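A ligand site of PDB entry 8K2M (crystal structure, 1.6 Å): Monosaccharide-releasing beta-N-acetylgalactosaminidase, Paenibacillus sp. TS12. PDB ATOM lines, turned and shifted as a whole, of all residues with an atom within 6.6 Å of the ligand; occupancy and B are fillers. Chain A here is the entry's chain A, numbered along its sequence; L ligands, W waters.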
ATOM      1  N   TRP A 199       8.386   3.459  23.863  1.00  0.00           N
ATOM      2  CA  TRP A 199       7.652   2.796  22.815  1.00  0.00           C
ATOM      3  C   TRP A 199       7.633   3.610  21.517  1.00  0.00           C
ATOM      4  O   TRP A 199       7.306   4.803  21.515  1.00  0.00           O
ATOM      5  CB  TRP A 199       6.242   2.394  23.261  1.00  0.00           C
ATOM      6  CG  TRP A 199       6.165   1.285  24.283  1.00  0.00           C
ATOM      7  CD1 TRP A 199       7.186   0.444  24.710  1.00  0.00           C
ATOM      8  CD2 TRP A 199       4.995   0.876  25.028  1.00  0.00           C
ATOM      9  NE1 TRP A 199       6.708  -0.450  25.650  1.00  0.00           N
ATOM     10  CE2 TRP A 199       5.367  -0.211  25.858  1.00  0.00           C
ATOM     11  CE3 TRP A 199       3.660   1.374  25.079  1.00  0.00           C
ATOM     12  CZ2 TRP A 199       4.456  -0.803  26.731  1.00  0.00           C
ATOM     13  CZ3 TRP A 199       2.758   0.750  25.924  1.00  0.00           C
ATOM     14  CH2 TRP A 199       3.155  -0.319  26.732  1.00  0.00           C
ATOM     15  N   LEU A 246      -2.542  -1.102  21.233  1.00  0.00           N
ATOM     16  CA  LEU A 246      -2.323  -0.004  22.171  1.00  0.00           C
ATOM     17  C   LEU A 246      -3.100   1.221  21.680  1.00  0.00           C
ATOM     18  O   LEU A 246      -3.109   1.519  20.481  1.00  0.00           O
ATOM     19  CB  LEU A 246      -0.842   0.335  22.318  1.00  0.00           C
ATOM     20  CG  LEU A 246       0.108  -0.810  22.703  1.00  0.00           C
ATOM     21  CD1 LEU A 246       1.547  -0.412  22.463  1.00  0.00           C
ATOM     22  CD2 LEU A 246      -0.116  -1.192  24.189  1.00  0.00           C
ATOM     23  N   ASP A 247      -3.712   1.948  22.608  1.00  0.00           N
ATOM     24  CA  ASP A 247      -4.386   3.236  22.354  1.00  0.00           C
ATOM     25  C   ASP A 247      -5.297   3.151  21.126  1.00  0.00           C
ATOM     26  O   ASP A 247      -5.231   4.030  20.231  1.00  0.00           O
ATOM     27  CB  ASP A 247      -3.381   4.404  22.267  1.00  0.00           C
ATOM     28  CG  ASP A 247      -2.670   4.607  23.603  1.00  0.00           C
ATOM     29  OD1 ASP A 247      -3.377   4.987  24.564  1.00  0.00           O
ATOM     30  OD2 ASP A 247      -1.481   4.207  23.698  1.00  0.00           O
ATOM     31  N   GLN A 300      -5.477  -4.249  24.897  1.00  0.00           N
ATOM     32  CA  GLN A 300      -5.214  -3.431  26.067  1.00  0.00           C
ATOM     33  C   GLN A 300      -6.416  -3.391  27.031  1.00  0.00           C
ATOM     34  O   GLN A 300      -7.568  -3.503  26.603  1.00  0.00           O
ATOM     35  CB  GLN A 300      -4.809  -2.012  25.618  1.00  0.00           C
ATOM     36  CG  GLN A 300      -4.254  -1.063  26.664  1.00  0.00           C
ATOM     37  CD  GLN A 300      -3.703   0.222  26.032  1.00  0.00           C
ATOM     38  OE1 GLN A 300      -4.269   0.703  25.031  1.00  0.00           O
ATOM     39  NE2 GLN A 300      -2.615   0.753  26.567  1.00  0.00           N
ATOM     40  N   TRP A 301      -6.130  -3.149  28.305  1.00  0.00           N
ATOM     41  CA  TRP A 301      -7.182  -2.844  29.292  1.00  0.00           C
ATOM     42  C   TRP A 301      -8.220  -3.991  29.328  1.00  0.00           C
ATOM     43  O   TRP A 301      -9.446  -3.756  29.303  1.00  0.00           O
ATOM     44  CB  TRP A 301      -7.851  -1.466  29.087  1.00  0.00           C
ATOM     45  CG  TRP A 301      -6.882  -0.306  29.051  1.00  0.00           C
ATOM     46  CD1 TRP A 301      -5.850  -0.061  29.892  1.00  0.00           C
ATOM     47  CD2 TRP A 301      -6.818   0.725  28.056  1.00  0.00           C
ATOM     48  NE1 TRP A 301      -5.151   1.063  29.501  1.00  0.00           N
ATOM     49  CE2 TRP A 301      -5.712   1.551  28.363  1.00  0.00           C
ATOM     50  CE3 TRP A 301      -7.565   0.981  26.897  1.00  0.00           C
ATOM     51  CZ2 TRP A 301      -5.399   2.687  27.618  1.00  0.00           C
ATOM     52  CZ3 TRP A 301      -7.243   2.107  26.159  1.00  0.00           C
ATOM     53  CH2 TRP A 301      -6.163   2.927  26.505  1.00  0.00           C
ATOM     54  N   ASP A 362      -1.341  -4.863  27.962  1.00  0.00           N
ATOM     55  CA  ASP A 362      -0.970  -3.713  28.763  1.00  0.00           C
ATOM     56  C   ASP A 362      -2.068  -3.275  29.757  1.00  0.00           C
ATOM     57  O   ASP A 362      -3.258  -3.281  29.425  1.00  0.00           O
ATOM     58  CB  ASP A 362      -0.640  -2.518  27.836  1.00  0.00           C
ATOM     59  CG  ASP A 362      -0.121  -1.299  28.562  1.00  0.00           C
ATOM     60  OD1 ASP A 362       0.867  -1.436  29.303  1.00  0.00           O
ATOM     61  OD2 ASP A 362      -0.685  -0.167  28.342  1.00  0.00           O
ATOM     62  N   GLU A 363      -1.643  -2.864  30.960  1.00  0.00           N
ATOM     63  CA  GLU A 363      -2.492  -2.189  31.962  1.00  0.00           C
ATOM     64  C   GLU A 363      -3.801  -2.947  32.297  1.00  0.00           C
ATOM     65  O   GLU A 363      -4.906  -2.368  32.279  1.00  0.00           O
ATOM     66  CB  GLU A 363      -2.759  -0.720  31.603  1.00  0.00           C
ATOM     67  CG  GLU A 363      -1.570   0.203  31.897  1.00  0.00           C
ATOM     68  CD  GLU A 363      -1.841   1.690  31.788  1.00  0.00           C
ATOM     69  OE1 GLU A 363      -2.822   2.047  31.034  1.00  0.00           O
ATOM     70  OE2 GLU A 363      -1.064   2.512  32.422  1.00  0.00           O
ATOM     71  N   ALA A 391       3.144  -3.412  32.173  1.00  0.00           N
ATOM     72  CA  ALA A 391       2.750  -2.292  33.006  1.00  0.00           C
ATOM     73  C   ALA A 391       1.423  -2.588  33.732  1.00  0.00           C
ATOM     74  O   ALA A 391       0.423  -2.952  33.126  1.00  0.00           O
ATOM     75  CB  ALA A 391       2.632  -1.025  32.174  1.00  0.00           C
ATOM     76  N   TYR A 427       7.461   2.907  35.490  1.00  0.00           N
ATOM     77  CA  TYR A 427       7.018   3.711  34.353  1.00  0.00           C
ATOM     78  C   TYR A 427       6.266   4.941  34.863  1.00  0.00           C
ATOM     79  O   TYR A 427       5.902   4.994  36.049  1.00  0.00           O
ATOM     80  CB  TYR A 427       6.074   2.970  33.386  1.00  0.00           C
ATOM     81  CG  TYR A 427       4.615   2.773  33.744  1.00  0.00           C
ATOM     82  CD1 TYR A 427       4.191   1.787  34.650  1.00  0.00           C
ATOM     83  CD2 TYR A 427       3.580   3.455  33.086  1.00  0.00           C
ATOM     84  CE1 TYR A 427       2.847   1.504  34.889  1.00  0.00           C
ATOM     85  CE2 TYR A 427       2.229   3.231  33.358  1.00  0.00           C
ATOM     86  CZ  TYR A 427       1.844   2.216  34.249  1.00  0.00           C
ATOM     87  OH  TYR A 427       0.483   1.910  34.430  1.00  0.00           O
ATOM     88  N   TYR A 428       6.001   5.925  33.961  1.00  0.00           N
ATOM     89  CA  TYR A 428       5.025   6.958  34.270  1.00  0.00           C
ATOM     90  C   TYR A 428       4.285   7.330  32.976  1.00  0.00           C
ATOM     91  O   TYR A 428       4.770   7.019  31.892  1.00  0.00           O
ATOM     92  CB  TYR A 428       5.653   8.153  34.991  1.00  0.00           C
ATOM     93  CG  TYR A 428       6.757   8.937  34.321  1.00  0.00           C
ATOM     94  CD1 TYR A 428       6.539   9.611  33.121  1.00  0.00           C
ATOM     95  CD2 TYR A 428       8.050   9.016  34.812  1.00  0.00           C
ATOM     96  CE1 TYR A 428       7.511  10.339  32.495  1.00  0.00           C
ATOM     97  CE2 TYR A 428       9.054   9.779  34.213  1.00  0.00           C
ATOM     98  CZ  TYR A 428       8.804  10.443  33.006  1.00  0.00           C
ATOM     99  OH  TYR A 428       9.774  11.208  32.344  1.00  0.00           O
ATOM    100  N   CYS A 429       3.127   8.038  33.123  1.00  0.00           N
ATOM    101  CA  CYS A 429       2.263   8.463  32.005  1.00  0.00           C
ATOM    102  C   CYS A 429       1.360   9.607  32.507  1.00  0.00           C
ATOM    103  O   CYS A 429       1.742  10.293  33.469  1.00  0.00           O
ATOM    104  CB  CYS A 429       1.485   7.274  31.455  1.00  0.00           C
ATOM    105  SG  CYS A 429       0.207   6.608  32.556  1.00  0.00           S
ATOM    106  N   CYS A 430       0.233   9.823  31.829  1.00  0.00           N
ATOM    107  CA  CYS A 430      -0.659  10.927  32.179  1.00  0.00           C
ATOM    108  C   CYS A 430      -1.182  10.795  33.611  1.00  0.00           C
ATOM    109  O   CYS A 430      -1.500  11.829  34.204  1.00  0.00           O
ATOM    110  CB  CYS A 430      -1.812  11.067  31.190  1.00  0.00           C
ATOM    111  SG  CYS A 430      -3.026   9.711  31.226  1.00  0.00           S
ATOM    112  N   GLY A 431      -1.230   9.576  34.156  1.00  0.00           N
ATOM    113  CA  GLY A 431      -1.814   9.336  35.478  1.00  0.00           C
ATOM    114  C   GLY A 431      -0.928   9.827  36.619  1.00  0.00           C
ATOM    115  O   GLY A 431      -1.436   9.997  37.759  1.00  0.00           O
ATOM    116  N   GLN A 432       0.363  10.039  36.329  1.00  0.00           N
ATOM    117  CA  GLN A 432       1.378  10.391  37.350  1.00  0.00           C
ATOM    118  C   GLN A 432       1.557  11.903  37.407  1.00  0.00           C
ATOM    119  O   GLN A 432       2.620  12.465  37.072  1.00  0.00           O
ATOM    120  CB  GLN A 432       2.671   9.614  37.098  1.00  0.00           C
ATOM    121  CG  GLN A 432       2.592   8.145  37.470  1.00  0.00           C
ATOM    122  CD  GLN A 432       1.614   7.344  36.661  1.00  0.00           C
ATOM    123  OE1 GLN A 432       1.734   7.256  35.443  1.00  0.00           O
ATOM    124  NE2 GLN A 432       0.632   6.744  37.333  1.00  0.00           N
ATOM    125  N   LEU A 464      10.335   2.163  31.668  1.00  0.00           N
ATOM    126  CA  LEU A 464       9.482   2.099  30.488  1.00  0.00           C
ATOM    127  C   LEU A 464       8.700   3.406  30.326  1.00  0.00           C
ATOM    128  O   LEU A 464       8.041   3.836  31.267  1.00  0.00           O
ATOM    129  CB  LEU A 464       8.544   0.880  30.646  1.00  0.00           C
ATOM    130  CG  LEU A 464       7.550   0.538  29.536  1.00  0.00           C
ATOM    131  CD1 LEU A 464       7.180  -0.963  29.478  1.00  0.00           C
ATOM    132  CD2 LEU A 464       6.260   1.336  29.691  1.00  0.00           C
ATOM    133  N   HIS A 465       8.575   3.890  29.085  1.00  0.00           N
ATOM    134  CA  HIS A 465       7.690   4.997  28.716  1.00  0.00           C
ATOM    135  C   HIS A 465       6.992   4.583  27.411  1.00  0.00           C
ATOM    136  O   HIS A 465       7.600   3.953  26.539  1.00  0.00           O
ATOM    137  CB  HIS A 465       8.452   6.333  28.631  1.00  0.00           C
ATOM    138  CG  HIS A 465       7.488   7.495  28.677  1.00  0.00           C
ATOM    139  ND1 HIS A 465       6.743   7.906  27.573  1.00  0.00           N
ATOM    140  CD2 HIS A 465       7.156   8.283  29.705  1.00  0.00           C
ATOM    141  CE1 HIS A 465       5.961   8.916  27.939  1.00  0.00           C
ATOM    142  NE2 HIS A 465       6.184   9.175  29.259  1.00  0.00           N
ATOM    143  N   TRP A 466       5.716   4.971  27.273  1.00  0.00           N
ATOM    144  CA  TRP A 466       4.834   4.633  26.163  1.00  0.00           C
ATOM    145  C   TRP A 466       5.001   5.564  24.950  1.00  0.00           C
ATOM    146  O   TRP A 466       4.407   5.231  23.894  1.00  0.00           O
ATOM    147  CB  TRP A 466       3.361   4.687  26.644  1.00  0.00           C
ATOM    148  CG  TRP A 466       2.818   6.084  26.801  1.00  0.00           C
ATOM    149  CD1 TRP A 466       2.998   6.995  27.812  1.00  0.00           C
ATOM    150  CD2 TRP A 466       1.955   6.743  25.841  1.00  0.00           C
ATOM    151  NE1 TRP A 466       2.330   8.154  27.547  1.00  0.00           N
ATOM    152  CE2 TRP A 466       1.639   8.001  26.370  1.00  0.00           C
ATOM    153  CE3 TRP A 466       1.328   6.324  24.625  1.00  0.00           C
ATOM    154  CZ2 TRP A 466       0.814   8.895  25.689  1.00  0.00           C
ATOM    155  CZ3 TRP A 466       0.519   7.199  23.956  1.00  0.00           C
ATOM    156  CH2 TRP A 466       0.254   8.465  24.494  1.00  0.00           C
ATOM    157  N   PHE A 492      -4.290  14.182  27.175  1.00  0.00           N
ATOM    158  CA  PHE A 492      -3.113  13.917  27.995  1.00  0.00           C
ATOM    159  C   PHE A 492      -2.355  15.225  28.203  1.00  0.00           C
ATOM    160  O   PHE A 492      -2.097  15.919  27.207  1.00  0.00           O
ATOM    161  CB  PHE A 492      -2.206  12.847  27.348  1.00  0.00           C
ATOM    162  CG  PHE A 492      -2.833  11.553  26.884  1.00  0.00           C
ATOM    163  CD1 PHE A 492      -3.760  10.871  27.707  1.00  0.00           C
ATOM    164  CD2 PHE A 492      -2.558  11.009  25.623  1.00  0.00           C
ATOM    165  CE1 PHE A 492      -4.340   9.677  27.299  1.00  0.00           C
ATOM    166  CE2 PHE A 492      -3.114   9.792  25.242  1.00  0.00           C
ATOM    167  CZ  PHE A 492      -4.045   9.151  26.051  1.00  0.00           C
ATOM    168  N   PRO A 493      -1.840  15.553  29.415  1.00  0.00           N
ATOM    169  CA  PRO A 493      -1.105  16.807  29.586  1.00  0.00           C
ATOM    170  C   PRO A 493       0.025  16.955  28.556  1.00  0.00           C
ATOM    171  O   PRO A 493       0.767  15.978  28.322  1.00  0.00           O
ATOM    172  CB  PRO A 493      -0.609  16.750  31.037  1.00  0.00           C
ATOM    173  CG  PRO A 493      -1.613  15.812  31.739  1.00  0.00           C
ATOM    174  CD  PRO A 493      -1.961  14.798  30.670  1.00  0.00           C
ATOM    175  N   ASP A 496       3.371  14.495  27.544  1.00  0.00           N
ATOM    176  CA  ASP A 496       3.170  13.057  27.761  1.00  0.00           C
ATOM    177  C   ASP A 496       3.314  12.228  26.467  1.00  0.00           C
ATOM    178  O   ASP A 496       4.051  11.228  26.439  1.00  0.00           O
ATOM    179  CB  ASP A 496       1.853  12.801  28.533  1.00  0.00           C
ATOM    180  CG  ASP A 496       1.507  11.326  28.746  1.00  0.00           C
ATOM    181  OD1 ASP A 496       2.343  10.582  29.306  1.00  0.00           O
ATOM    182  OD2 ASP A 496       0.412  10.923  28.330  1.00  0.00           O
ATOM    183  N   PRO A 497       2.640  12.522  25.333  1.00  0.00           N
ATOM    184  CA  PRO A 497       2.665  11.553  24.235  1.00  0.00           C
ATOM    185  C   PRO A 497       3.916  11.489  23.360  1.00  0.00           C
ATOM    186  O   PRO A 497       4.106  10.488  22.670  1.00  0.00           O
ATOM    187  CB  PRO A 497       1.449  11.958  23.358  1.00  0.00           C
ATOM    188  CG  PRO A 497       1.231  13.421  23.674  1.00  0.00           C
ATOM    189  CD  PRO A 497       1.583  13.545  25.157  1.00  0.00           C
HETATM  190  C1  LIG L   1      -0.506   4.449  29.691  1.00  0.00           C
HETATM  191  S1  LIG L   1       1.312   4.298  29.942  1.00  0.00           S
HETATM  192  C2  LIG L   1      -0.834   3.467  28.566  1.00  0.00           C
HETATM  193  N1  LIG L   1       0.049   2.285  28.781  1.00  0.00           N
HETATM  194  C3  LIG L   1      -0.524   4.066  27.179  1.00  0.00           C
HETATM  195  O1  LIG L   1      -0.949   3.141  26.169  1.00  0.00           O
HETATM  196  C4  LIG L   1      -1.207   5.458  27.120  1.00  0.00           C
HETATM  197  O2  LIG L   1      -2.660   5.387  27.097  1.00  0.00           O
HETATM  198  C5  LIG L   1      -0.738   6.359  28.255  1.00  0.00           C
HETATM  199  O3  LIG L   1      -1.006   5.762  29.545  1.00  0.00           O
HETATM  200  C6  LIG L   1      -1.369   7.749  28.282  1.00  0.00           C
HETATM  201  O4  LIG L   1      -0.668   8.594  29.174  1.00  0.00           O
HETATM  202  C7  LIG L   1       1.119   2.654  29.397  1.00  0.00           C
HETATM  203  C8  LIG L   1       2.255   1.746  29.716  1.00  0.00           C
HETATM  204  O   HOH W   1      -4.707   6.107  28.738  1.00  0.00           O
HETATM  205  O   HOH W   2       4.677   4.915  30.014  1.00  0.00           O
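Water W2 lies within hydrogen-bond range of O of Tyr 428 (2.8 Å), N of Trp 466 (2.9 Å) and S1 of the ligand (3.4 Å).
The backbone NH of Cys 429 lies within hydrogen-bond range of the side-chain amide oxygen of Gln 432 (2.8 Å).
The side-chain carboxylate of Asp 496 sits at hydrogen-bond distance from the backbone NH of Cys 430, 3.4 Å away.
OE1 of Gln 300 sits at hydrogen-bond distance from N of Asp 247 (2.8 Å).
NE2 of Gln 300 is in hydrogen-bond range of OD2 of Asp 362 (2.8 Å).
OD1 of Asp 496 lies within hydrogen-bond range of NE1 of Trp 466, at 3.0 Å.
O of Asp 362 lies within hydrogen-bond range of N of Trp 301, 3.1 Å away.
N of Trp 199 sits at hydrogen-bond distance from O of His 465 (2.8 Å).
The side-chain sulfur (SG) of Cys 429 lies close to the backbone NH (N) of Gly 431.
The side-chain sulfur (SG) of Cys 429 sits at hydrogen-bond distance from an oxygen (O3) of the ligand (3.4 Å).
NE2 of Gln 300 sits at hydrogen-bond distance from O1 of the ligand, at 2.9 Å.
The side-chain carboxylate (OD2) of Asp 362 lies within hydrogen-bond range of a nitrogen (N1) of the ligand.
The backbone NH (N) of Cys 430 sits at hydrogen-bond distance from an oxygen (O4) of the ligand.
OD1 of Asp 247 is in hydrogen-bond range of O2 of the ligand, 2.7 Å away.
An oxygen (O4) of the ligand is in hydrogen-bond range of the side-chain carboxylate (OD2) of Asp 496 (2.7 Å).
O4 of the ligand lies within hydrogen-bond range of SG of Cys 430.
NE1 of Trp 466 lies within hydrogen-bond range of O4 of the ligand (3.4 Å).
Trp 199 touches the ligand.
Trp 301 touches the ligand (CZ2 to O2, 3.9 Å).
Glu 363 touches the ligand.
CB of Ala 391 touches C8 of the ligand (3.7 Å).
Tyr 427 touches the ligand (CE2 to S1, 3.7 Å).
Phe 492 touches the ligand (CE1 to C6, 3.7 Å).
The nearest printed residue that does not touch the ligand is Leu 464 (4.03 Å).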
